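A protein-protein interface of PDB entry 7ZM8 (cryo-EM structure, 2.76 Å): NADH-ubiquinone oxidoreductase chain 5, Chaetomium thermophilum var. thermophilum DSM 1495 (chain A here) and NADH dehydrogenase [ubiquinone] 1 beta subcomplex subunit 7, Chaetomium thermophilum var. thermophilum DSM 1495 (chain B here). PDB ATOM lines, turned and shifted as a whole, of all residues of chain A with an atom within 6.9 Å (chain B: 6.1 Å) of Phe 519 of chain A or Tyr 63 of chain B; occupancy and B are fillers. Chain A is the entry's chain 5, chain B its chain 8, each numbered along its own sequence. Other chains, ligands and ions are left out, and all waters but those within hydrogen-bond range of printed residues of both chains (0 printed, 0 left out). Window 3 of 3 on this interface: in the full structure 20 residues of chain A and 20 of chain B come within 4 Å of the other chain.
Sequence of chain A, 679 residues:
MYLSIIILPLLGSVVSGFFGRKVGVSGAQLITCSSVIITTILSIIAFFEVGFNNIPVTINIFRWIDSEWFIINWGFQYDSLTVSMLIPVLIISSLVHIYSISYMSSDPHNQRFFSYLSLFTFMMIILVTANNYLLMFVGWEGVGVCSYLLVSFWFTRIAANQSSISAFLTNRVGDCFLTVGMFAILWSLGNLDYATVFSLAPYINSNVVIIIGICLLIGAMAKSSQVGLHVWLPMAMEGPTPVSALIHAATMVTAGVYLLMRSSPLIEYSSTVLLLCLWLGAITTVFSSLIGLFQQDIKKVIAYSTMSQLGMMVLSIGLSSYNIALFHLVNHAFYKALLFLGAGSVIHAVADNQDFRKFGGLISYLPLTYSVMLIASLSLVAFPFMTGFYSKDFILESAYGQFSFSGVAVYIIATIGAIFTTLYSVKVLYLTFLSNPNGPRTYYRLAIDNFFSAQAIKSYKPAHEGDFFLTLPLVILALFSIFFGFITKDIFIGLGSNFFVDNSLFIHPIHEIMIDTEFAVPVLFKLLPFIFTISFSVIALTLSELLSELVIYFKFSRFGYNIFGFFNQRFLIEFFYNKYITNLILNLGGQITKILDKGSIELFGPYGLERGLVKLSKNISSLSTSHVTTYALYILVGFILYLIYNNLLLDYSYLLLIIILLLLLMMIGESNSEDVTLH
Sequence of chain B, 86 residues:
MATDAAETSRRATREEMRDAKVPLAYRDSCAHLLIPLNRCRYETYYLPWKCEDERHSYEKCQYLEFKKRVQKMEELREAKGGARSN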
ATOM      1  N   LEU A 495      -3.700  -7.275   6.866  1.00  0.00           N
ATOM      2  CA  LEU A 495      -2.803  -8.337   7.294  1.00  0.00           C
ATOM      3  C   LEU A 495      -2.511  -8.266   8.783  1.00  0.00           C
ATOM      4  O   LEU A 495      -2.404  -9.305   9.436  1.00  0.00           O
ATOM      5  CB  LEU A 495      -1.500  -8.296   6.498  1.00  0.00           C
ATOM      6  CG  LEU A 495      -0.605  -9.512   6.720  1.00  0.00           C
ATOM      7  CD1 LEU A 495      -1.419 -10.784   6.593  1.00  0.00           C
ATOM      8  CD2 LEU A 495       0.550  -9.517   5.739  1.00  0.00           C
ATOM      9  N   MET A 514      -4.217 -16.589   9.236  1.00  0.00           N
ATOM     10  CA  MET A 514      -4.136 -15.571   8.199  1.00  0.00           C
ATOM     11  C   MET A 514      -2.833 -15.667   7.421  1.00  0.00           C
ATOM     12  O   MET A 514      -2.827 -15.548   6.191  1.00  0.00           O
ATOM     13  CB  MET A 514      -4.276 -14.189   8.831  1.00  0.00           C
ATOM     14  CG  MET A 514      -4.326 -13.040   7.840  1.00  0.00           C
ATOM     15  SD  MET A 514      -5.773 -13.134   6.779  1.00  0.00           S
ATOM     16  CE  MET A 514      -7.060 -12.683   7.938  1.00  0.00           C
ATOM     17  N   ILE A 515      -1.717 -15.871   8.121  1.00  0.00           N
ATOM     18  CA  ILE A 515      -0.409 -15.822   7.478  1.00  0.00           C
ATOM     19  C   ILE A 515      -0.212 -17.025   6.567  1.00  0.00           C
ATOM     20  O   ILE A 515       0.389 -16.915   5.494  1.00  0.00           O
ATOM     21  CB  ILE A 515       0.699 -15.731   8.540  1.00  0.00           C
ATOM     22  CG1 ILE A 515       0.467 -14.521   9.443  1.00  0.00           C
ATOM     23  CG2 ILE A 515       2.056 -15.618   7.878  1.00  0.00           C
ATOM     24  CD1 ILE A 515       1.496 -14.373  10.533  1.00  0.00           C
ATOM     25  N   ASP A 516      -0.695 -18.196   6.984  1.00  0.00           N
ATOM     26  CA  ASP A 516      -0.642 -19.365   6.116  1.00  0.00           C
ATOM     27  C   ASP A 516      -1.575 -19.208   4.922  1.00  0.00           C
ATOM     28  O   ASP A 516      -1.243 -19.624   3.810  1.00  0.00           O
ATOM     29  CB  ASP A 516      -0.989 -20.622   6.908  1.00  0.00           C
ATOM     30  CG  ASP A 516       0.078 -20.987   7.924  1.00  0.00           C
ATOM     31  OD1 ASP A 516       1.264 -20.671   7.689  1.00  0.00           O
ATOM     32  OD2 ASP A 516      -0.269 -21.591   8.961  1.00  0.00           O
ATOM     33  N   THR A 517      -2.749 -18.613   5.131  1.00  0.00           N
ATOM     34  CA  THR A 517      -3.660 -18.383   4.018  1.00  0.00           C
ATOM     35  C   THR A 517      -3.047 -17.442   2.991  1.00  0.00           C
ATOM     36  O   THR A 517      -3.355 -17.537   1.798  1.00  0.00           O
ATOM     37  CB  THR A 517      -4.989 -17.834   4.535  1.00  0.00           C
ATOM     38  OG1 THR A 517      -5.534 -18.742   5.498  1.00  0.00           O
ATOM     39  CG2 THR A 517      -5.980 -17.665   3.406  1.00  0.00           C
ATOM     40  N   GLU A 518      -2.171 -16.540   3.431  1.00  0.00           N
ATOM     41  CA  GLU A 518      -1.493 -15.637   2.509  1.00  0.00           C
ATOM     42  C   GLU A 518      -0.367 -16.326   1.752  1.00  0.00           C
ATOM     43  O   GLU A 518      -0.113 -15.987   0.592  1.00  0.00           O
ATOM     44  CB  GLU A 518      -0.947 -14.430   3.272  1.00  0.00           C
ATOM     45  CG  GLU A 518      -0.378 -13.331   2.389  1.00  0.00           C
ATOM     46  CD  GLU A 518      -1.433 -12.655   1.531  1.00  0.00           C
ATOM     47  OE1 GLU A 518      -2.616 -12.638   1.934  1.00  0.00           O
ATOM     48  OE2 GLU A 518      -1.078 -12.136   0.452  1.00  0.00           O
ATOM     49  N   PHE A 519       0.307 -17.288   2.373  1.00  0.00           N
ATOM     50  CA  PHE A 519       1.540 -17.840   1.830  1.00  0.00           C
ATOM     51  C   PHE A 519       1.503 -19.342   1.618  1.00  0.00           C
ATOM     52  O   PHE A 519       2.057 -19.829   0.632  1.00  0.00           O
ATOM     53  CB  PHE A 519       2.714 -17.503   2.754  1.00  0.00           C
ATOM     54  CG  PHE A 519       2.939 -16.034   2.948  1.00  0.00           C
ATOM     55  CD1 PHE A 519       2.895 -15.165   1.879  1.00  0.00           C
ATOM     56  CD2 PHE A 519       3.208 -15.524   4.207  1.00  0.00           C
ATOM     57  CE1 PHE A 519       3.105 -13.817   2.063  1.00  0.00           C
ATOM     58  CE2 PHE A 519       3.417 -14.175   4.393  1.00  0.00           C
ATOM     59  CZ  PHE A 519       3.368 -13.323   3.321  1.00  0.00           C
ATOM     60  N   ALA A 520       0.878 -20.094   2.524  1.00  0.00           N
ATOM     61  CA  ALA A 520       0.954 -21.550   2.464  1.00  0.00           C
ATOM     62  C   ALA A 520       0.091 -22.131   1.356  1.00  0.00           C
ATOM     63  O   ALA A 520       0.512 -23.069   0.673  1.00  0.00           O
ATOM     64  CB  ALA A 520       0.554 -22.153   3.808  1.00  0.00           C
ATOM     65  N   VAL A 521      -1.109 -21.592   1.166  1.00  0.00           N
ATOM     66  CA  VAL A 521      -2.069 -22.198   0.237  1.00  0.00           C
ATOM     67  C   VAL A 521      -1.496 -22.164  -1.173  1.00  0.00           C
ATOM     68  O   VAL A 521      -1.003 -21.110  -1.616  1.00  0.00           O
ATOM     69  CB  VAL A 521      -3.419 -21.468   0.304  1.00  0.00           C
ATOM     70  CG1 VAL A 521      -4.387 -22.022  -0.720  1.00  0.00           C
ATOM     71  CG2 VAL A 521      -4.005 -21.587   1.690  1.00  0.00           C
ATOM     72  N   PRO A 522      -1.510 -23.273  -1.906  1.00  0.00           N
ATOM     73  CA  PRO A 522      -0.952 -23.271  -3.259  1.00  0.00           C
ATOM     74  C   PRO A 522      -1.801 -22.448  -4.210  1.00  0.00           C
ATOM     75  O   PRO A 522      -2.982 -22.185  -3.976  1.00  0.00           O
ATOM     76  CB  PRO A 522      -0.958 -24.752  -3.648  1.00  0.00           C
ATOM     77  CG  PRO A 522      -2.014 -25.356  -2.803  1.00  0.00           C
ATOM     78  CD  PRO A 522      -1.997 -24.605  -1.512  1.00  0.00           C
ATOM     79  N   LYS A 526      -5.885 -21.761  -4.773  1.00  0.00           N
ATOM     80  CA  LYS A 526      -6.249 -20.352  -4.736  1.00  0.00           C
ATOM     81  C   LYS A 526      -7.019 -19.953  -5.986  1.00  0.00           C
ATOM     82  O   LYS A 526      -7.976 -19.175  -5.913  1.00  0.00           O
ATOM     83  CB  LYS A 526      -4.996 -19.495  -4.579  1.00  0.00           C
ATOM     84  CG  LYS A 526      -4.521 -19.364  -3.146  1.00  0.00           C
ATOM     85  CD  LYS A 526      -3.277 -18.502  -3.057  1.00  0.00           C
ATOM     86  CE  LYS A 526      -3.010 -18.064  -1.627  1.00  0.00           C
ATOM     87  NZ  LYS A 526      -1.930 -17.042  -1.558  1.00  0.00           N
ATOM     88  N   TYR B  58       6.058  -4.986   5.612  1.00  0.00           N
ATOM     89  CA  TYR B  58       5.413  -5.899   6.545  1.00  0.00           C
ATOM     90  C   TYR B  58       5.077  -7.222   5.874  1.00  0.00           C
ATOM     91  O   TYR B  58       5.278  -8.292   6.457  1.00  0.00           O
ATOM     92  CB  TYR B  58       4.150  -5.269   7.126  1.00  0.00           C
ATOM     93  CG  TYR B  58       3.560  -6.088   8.247  1.00  0.00           C
ATOM     94  CD1 TYR B  58       4.300  -6.370   9.380  1.00  0.00           C
ATOM     95  CD2 TYR B  58       2.278  -6.603   8.159  1.00  0.00           C
ATOM     96  CE1 TYR B  58       3.778  -7.123  10.400  1.00  0.00           C
ATOM     97  CE2 TYR B  58       1.747  -7.360   9.180  1.00  0.00           C
ATOM     98  CZ  TYR B  58       2.506  -7.616  10.296  1.00  0.00           C
ATOM     99  OH  TYR B  58       1.989  -8.368  11.319  1.00  0.00           O
ATOM    100  N   GLU B  59       4.552  -7.169   4.649  1.00  0.00           N
ATOM    101  CA  GLU B  59       4.239  -8.398   3.931  1.00  0.00           C
ATOM    102  C   GLU B  59       5.497  -9.184   3.608  1.00  0.00           C
ATOM    103  O   GLU B  59       5.521 -10.411   3.755  1.00  0.00           O
ATOM    104  CB  GLU B  59       3.468  -8.074   2.655  1.00  0.00           C
ATOM    105  CG  GLU B  59       2.008  -7.720   2.882  1.00  0.00           C
ATOM    106  CD  GLU B  59       1.426  -6.912   1.743  1.00  0.00           C
ATOM    107  OE1 GLU B  59       0.209  -6.631   1.770  1.00  0.00           O
ATOM    108  OE2 GLU B  59       2.188  -6.554   0.821  1.00  0.00           O
ATOM    109  N   LYS B  60       6.553  -8.500   3.160  1.00  0.00           N
ATOM    110  CA  LYS B  60       7.799  -9.185   2.842  1.00  0.00           C
ATOM    111  C   LYS B  60       8.394  -9.849   4.072  1.00  0.00           C
ATOM    112  O   LYS B  60       8.830 -11.001   4.011  1.00  0.00           O
ATOM    113  CB  LYS B  60       8.804  -8.205   2.243  1.00  0.00           C
ATOM    114  CG  LYS B  60      10.092  -8.852   1.786  1.00  0.00           C
ATOM    115  CD  LYS B  60      11.014  -7.843   1.126  1.00  0.00           C
ATOM    116  CE  LYS B  60      12.310  -8.492   0.676  1.00  0.00           C
ATOM    117  NZ  LYS B  60      13.221  -7.508   0.030  1.00  0.00           N
ATOM    118  N   CYS B  61       8.419  -9.138   5.201  1.00  0.00           N
ATOM    119  CA  CYS B  61       9.048  -9.689   6.396  1.00  0.00           C
ATOM    120  C   CYS B  61       8.325 -10.944   6.864  1.00  0.00           C
ATOM    121  O   CYS B  61       8.958 -11.973   7.113  1.00  0.00           O
ATOM    122  CB  CYS B  61       9.082  -8.636   7.502  1.00  0.00           C
ATOM    123  SG  CYS B  61       9.907  -9.177   9.015  1.00  0.00           S
ATOM    124  N   GLN B  62       6.995 -10.889   6.941  1.00  0.00           N
ATOM    125  CA  GLN B  62       6.211 -12.062   7.308  1.00  0.00           C
ATOM    126  C   GLN B  62       6.491 -13.241   6.394  1.00  0.00           C
ATOM    127  O   GLN B  62       6.361 -14.395   6.814  1.00  0.00           O
ATOM    128  CB  GLN B  62       4.724 -11.719   7.273  1.00  0.00           C
ATOM    129  CG  GLN B  62       4.247 -10.893   8.433  1.00  0.00           C
ATOM    130  CD  GLN B  62       3.969 -11.733   9.656  1.00  0.00           C
ATOM    131  OE1 GLN B  62       4.750 -12.611  10.017  1.00  0.00           O
ATOM    132  NE2 GLN B  62       2.861 -11.445  10.325  1.00  0.00           N
ATOM    133  N   TYR B  63       6.861 -12.969   5.146  1.00  0.00           N
ATOM    134  CA  TYR B  63       7.177 -14.068   4.201  1.00  0.00           C
ATOM    135  C   TYR B  63       8.443 -14.774   4.668  1.00  0.00           C
ATOM    136  O   TYR B  63       8.474 -16.006   4.620  1.00  0.00           O
ATOM    137  CB  TYR B  63       7.332 -13.545   2.774  1.00  0.00           C
ATOM    138  CG  TYR B  63       7.474 -14.624   1.731  1.00  0.00           C
ATOM    139  CD1 TYR B  63       6.458 -15.538   1.509  1.00  0.00           C
ATOM    140  CD2 TYR B  63       8.622 -14.731   0.966  1.00  0.00           C
ATOM    141  CE1 TYR B  63       6.578 -16.532   0.553  1.00  0.00           C
ATOM    142  CE2 TYR B  63       8.758 -15.719   0.006  1.00  0.00           C
ATOM    143  CZ  TYR B  63       7.732 -16.621  -0.202  1.00  0.00           C
ATOM    144  OH  TYR B  63       7.860 -17.599  -1.145  1.00  0.00           O
ATOM    145  N   LEU B  64       9.434 -14.015   5.132  1.00  0.00           N
ATOM    146  CA  LEU B  64      10.712 -14.609   5.515  1.00  0.00           C
ATOM    147  C   LEU B  64      10.574 -15.565   6.694  1.00  0.00           C
ATOM    148  O   LEU B  64      11.182 -16.640   6.691  1.00  0.00           O
ATOM    149  CB  LEU B  64      11.738 -13.519   5.832  1.00  0.00           C
ATOM    150  CG  LEU B  64      12.525 -12.862   4.691  1.00  0.00           C
ATOM    151  CD1 LEU B  64      13.408 -13.891   4.000  1.00  0.00           C
ATOM    152  CD2 LEU B  64      11.634 -12.180   3.676  1.00  0.00           C
ATOM    153  N   GLU B  65       9.805 -15.193   7.723  1.00  0.00           N
ATOM    154  CA  GLU B  65       9.642 -16.112   8.844  1.00  0.00           C
ATOM    155  C   GLU B  65       8.747 -17.283   8.479  1.00  0.00           C
ATOM    156  O   GLU B  65       8.888 -18.374   9.044  1.00  0.00           O
ATOM    157  CB  GLU B  65       9.104 -15.402  10.088  1.00  0.00           C
ATOM    158  CG  GLU B  65      10.115 -14.518  10.799  1.00  0.00           C
ATOM    159  CD  GLU B  65      10.111 -13.107  10.294  1.00  0.00           C
ATOM    160  OE1 GLU B  65       9.220 -12.792   9.490  1.00  0.00           O
ATOM    161  OE2 GLU B  65      10.992 -12.316  10.694  1.00  0.00           O
ATOM    162  N   PHE B  66       7.818 -17.085   7.549  1.00  0.00           N
ATOM    163  CA  PHE B  66       7.056 -18.221   7.051  1.00  0.00           C
ATOM    164  C   PHE B  66       7.975 -19.218   6.367  1.00  0.00           C
ATOM    165  O   PHE B  66       7.867 -20.427   6.590  1.00  0.00           O
ATOM    166  CB  PHE B  66       5.967 -17.737   6.093  1.00  0.00           C
ATOM    167  CG  PHE B  66       5.306 -18.833   5.327  1.00  0.00           C
ATOM    168  CD1 PHE B  66       4.321 -19.606   5.911  1.00  0.00           C
ATOM    169  CD2 PHE B  66       5.663 -19.090   4.022  1.00  0.00           C
ATOM    170  CE1 PHE B  66       3.708 -20.614   5.204  1.00  0.00           C
ATOM    171  CE2 PHE B  66       5.058 -20.093   3.317  1.00  0.00           C
ATOM    172  CZ  PHE B  66       4.079 -20.856   3.907  1.00  0.00           C
ATOM    173  N   LYS B  67       8.910 -18.724   5.556  1.00  0.00           N
ATOM    174  CA  LYS B  67       9.854 -19.608   4.888  1.00  0.00           C
ATOM    175  C   LYS B  67      10.724 -20.354   5.892  1.00  0.00           C
ATOM    176  O   LYS B  67      10.981 -21.551   5.732  1.00  0.00           O
ATOM    177  CB  LYS B  67      10.718 -18.809   3.916  1.00  0.00           C
ATOM    178  CG  LYS B  67       9.937 -18.131   2.809  1.00  0.00           C
ATOM    179  CD  LYS B  67       9.221 -19.150   1.942  1.00  0.00           C
ATOM    180  CE  LYS B  67      10.209 -20.002   1.162  1.00  0.00           C
ATOM    181  NZ  LYS B  67      10.988 -19.196   0.181  1.00  0.00           N
ATOM    182  N   LYS B  68      11.193 -19.664   6.936  1.00  0.00           N
ATOM    183  CA  LYS B  68      11.963 -20.353   7.964  1.00  0.00           C
ATOM    184  C   LYS B  68      11.127 -21.397   8.691  1.00  0.00           C
ATOM    185  O   LYS B  68      11.647 -22.455   9.055  1.00  0.00           O
ATOM    186  CB  LYS B  68      12.559 -19.358   8.960  1.00  0.00           C
ATOM    187  CG  LYS B  68      13.578 -18.402   8.354  1.00  0.00           C
ATOM    188  CD  LYS B  68      14.196 -17.486   9.410  1.00  0.00           C
ATOM    189  CE  LYS B  68      13.230 -16.444   9.944  1.00  0.00           C
ATOM    190  NZ  LYS B  68      12.845 -15.463   8.900  1.00  0.00           N
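OH of Tyr 58 of chain B is in hydrogen-bond range of NE2 of Gln 62 of chain B (3.3 Å). The backbone carbonyl oxygen (O) of Asp 516 of chain A sits at hydrogen-bond distance from the backbone NH (N) of Val 521 of chain A.
Among the printed residues, merely in contact across the chains: Ile 515 of chain A with Gln 62 of chain B (3.2 Å), Asp 516 of chain A with Phe 66 of chain B (3.5 Å), Ala 520 of chain A with Phe 66 of chain B (3.5 Å), Phe 519 of chain A with Phe 66 of chain B (3.5 Å), Phe 519 of chain A with Tyr 63 of chain B (3.6 Å), Phe 519 of chain A with Glu 59 of chain B (3.6 Å), Leu 495 of chain A with Glu 59 of chain B (3.7 Å) and Phe 519 of chain A with Gln 62 of chain B (3.8 Å).
Of chain A, only Phe 519 comes within 4 Å of Tyr 63 of chain B. Printed residues of chain B within 4 Å of Asp 516 of chain A: Phe 66. Printed residues of chain B within 4 Å of Ala 520 of chain A: Phe 66. Of the printed residues of chain B, Ile 515 of chain A touches Gln 62 (3.2 Å). Printed residues of chain A within 4 Å of Phe 66 of chain B: Asp 516 (3.5 Å), Phe 519 (3.5 Å) and Ala 520 (3.5 Å). The nearest residue of chain A that does not touch Tyr 63 of chain B is Ile 515 of chain A (6.1 Å).
Of the 11 printed residues of chain A, 5 touch a printed residue of chain B. Printed residues of chain A that touch a printed residue of chain B: Leu 495, Ile 515, Asp 516, Phe 519 and Ala 520. Hydrophobic or aromatic side chains of chain A that line the printed part of chain B: Leu 495, Ile 515, Phe 519 and Ala 520. Hydrophobic or aromatic side chains of chain B within 4 Å of the printed part of chain A: Tyr 63 and Phe 66. Among the printed residues, 8 pairs touch across the chains. Among the printed residues, no Asp or Glu carboxylate lies within 4 Å of a Lys or Arg side-chain nitrogen of the other chain.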
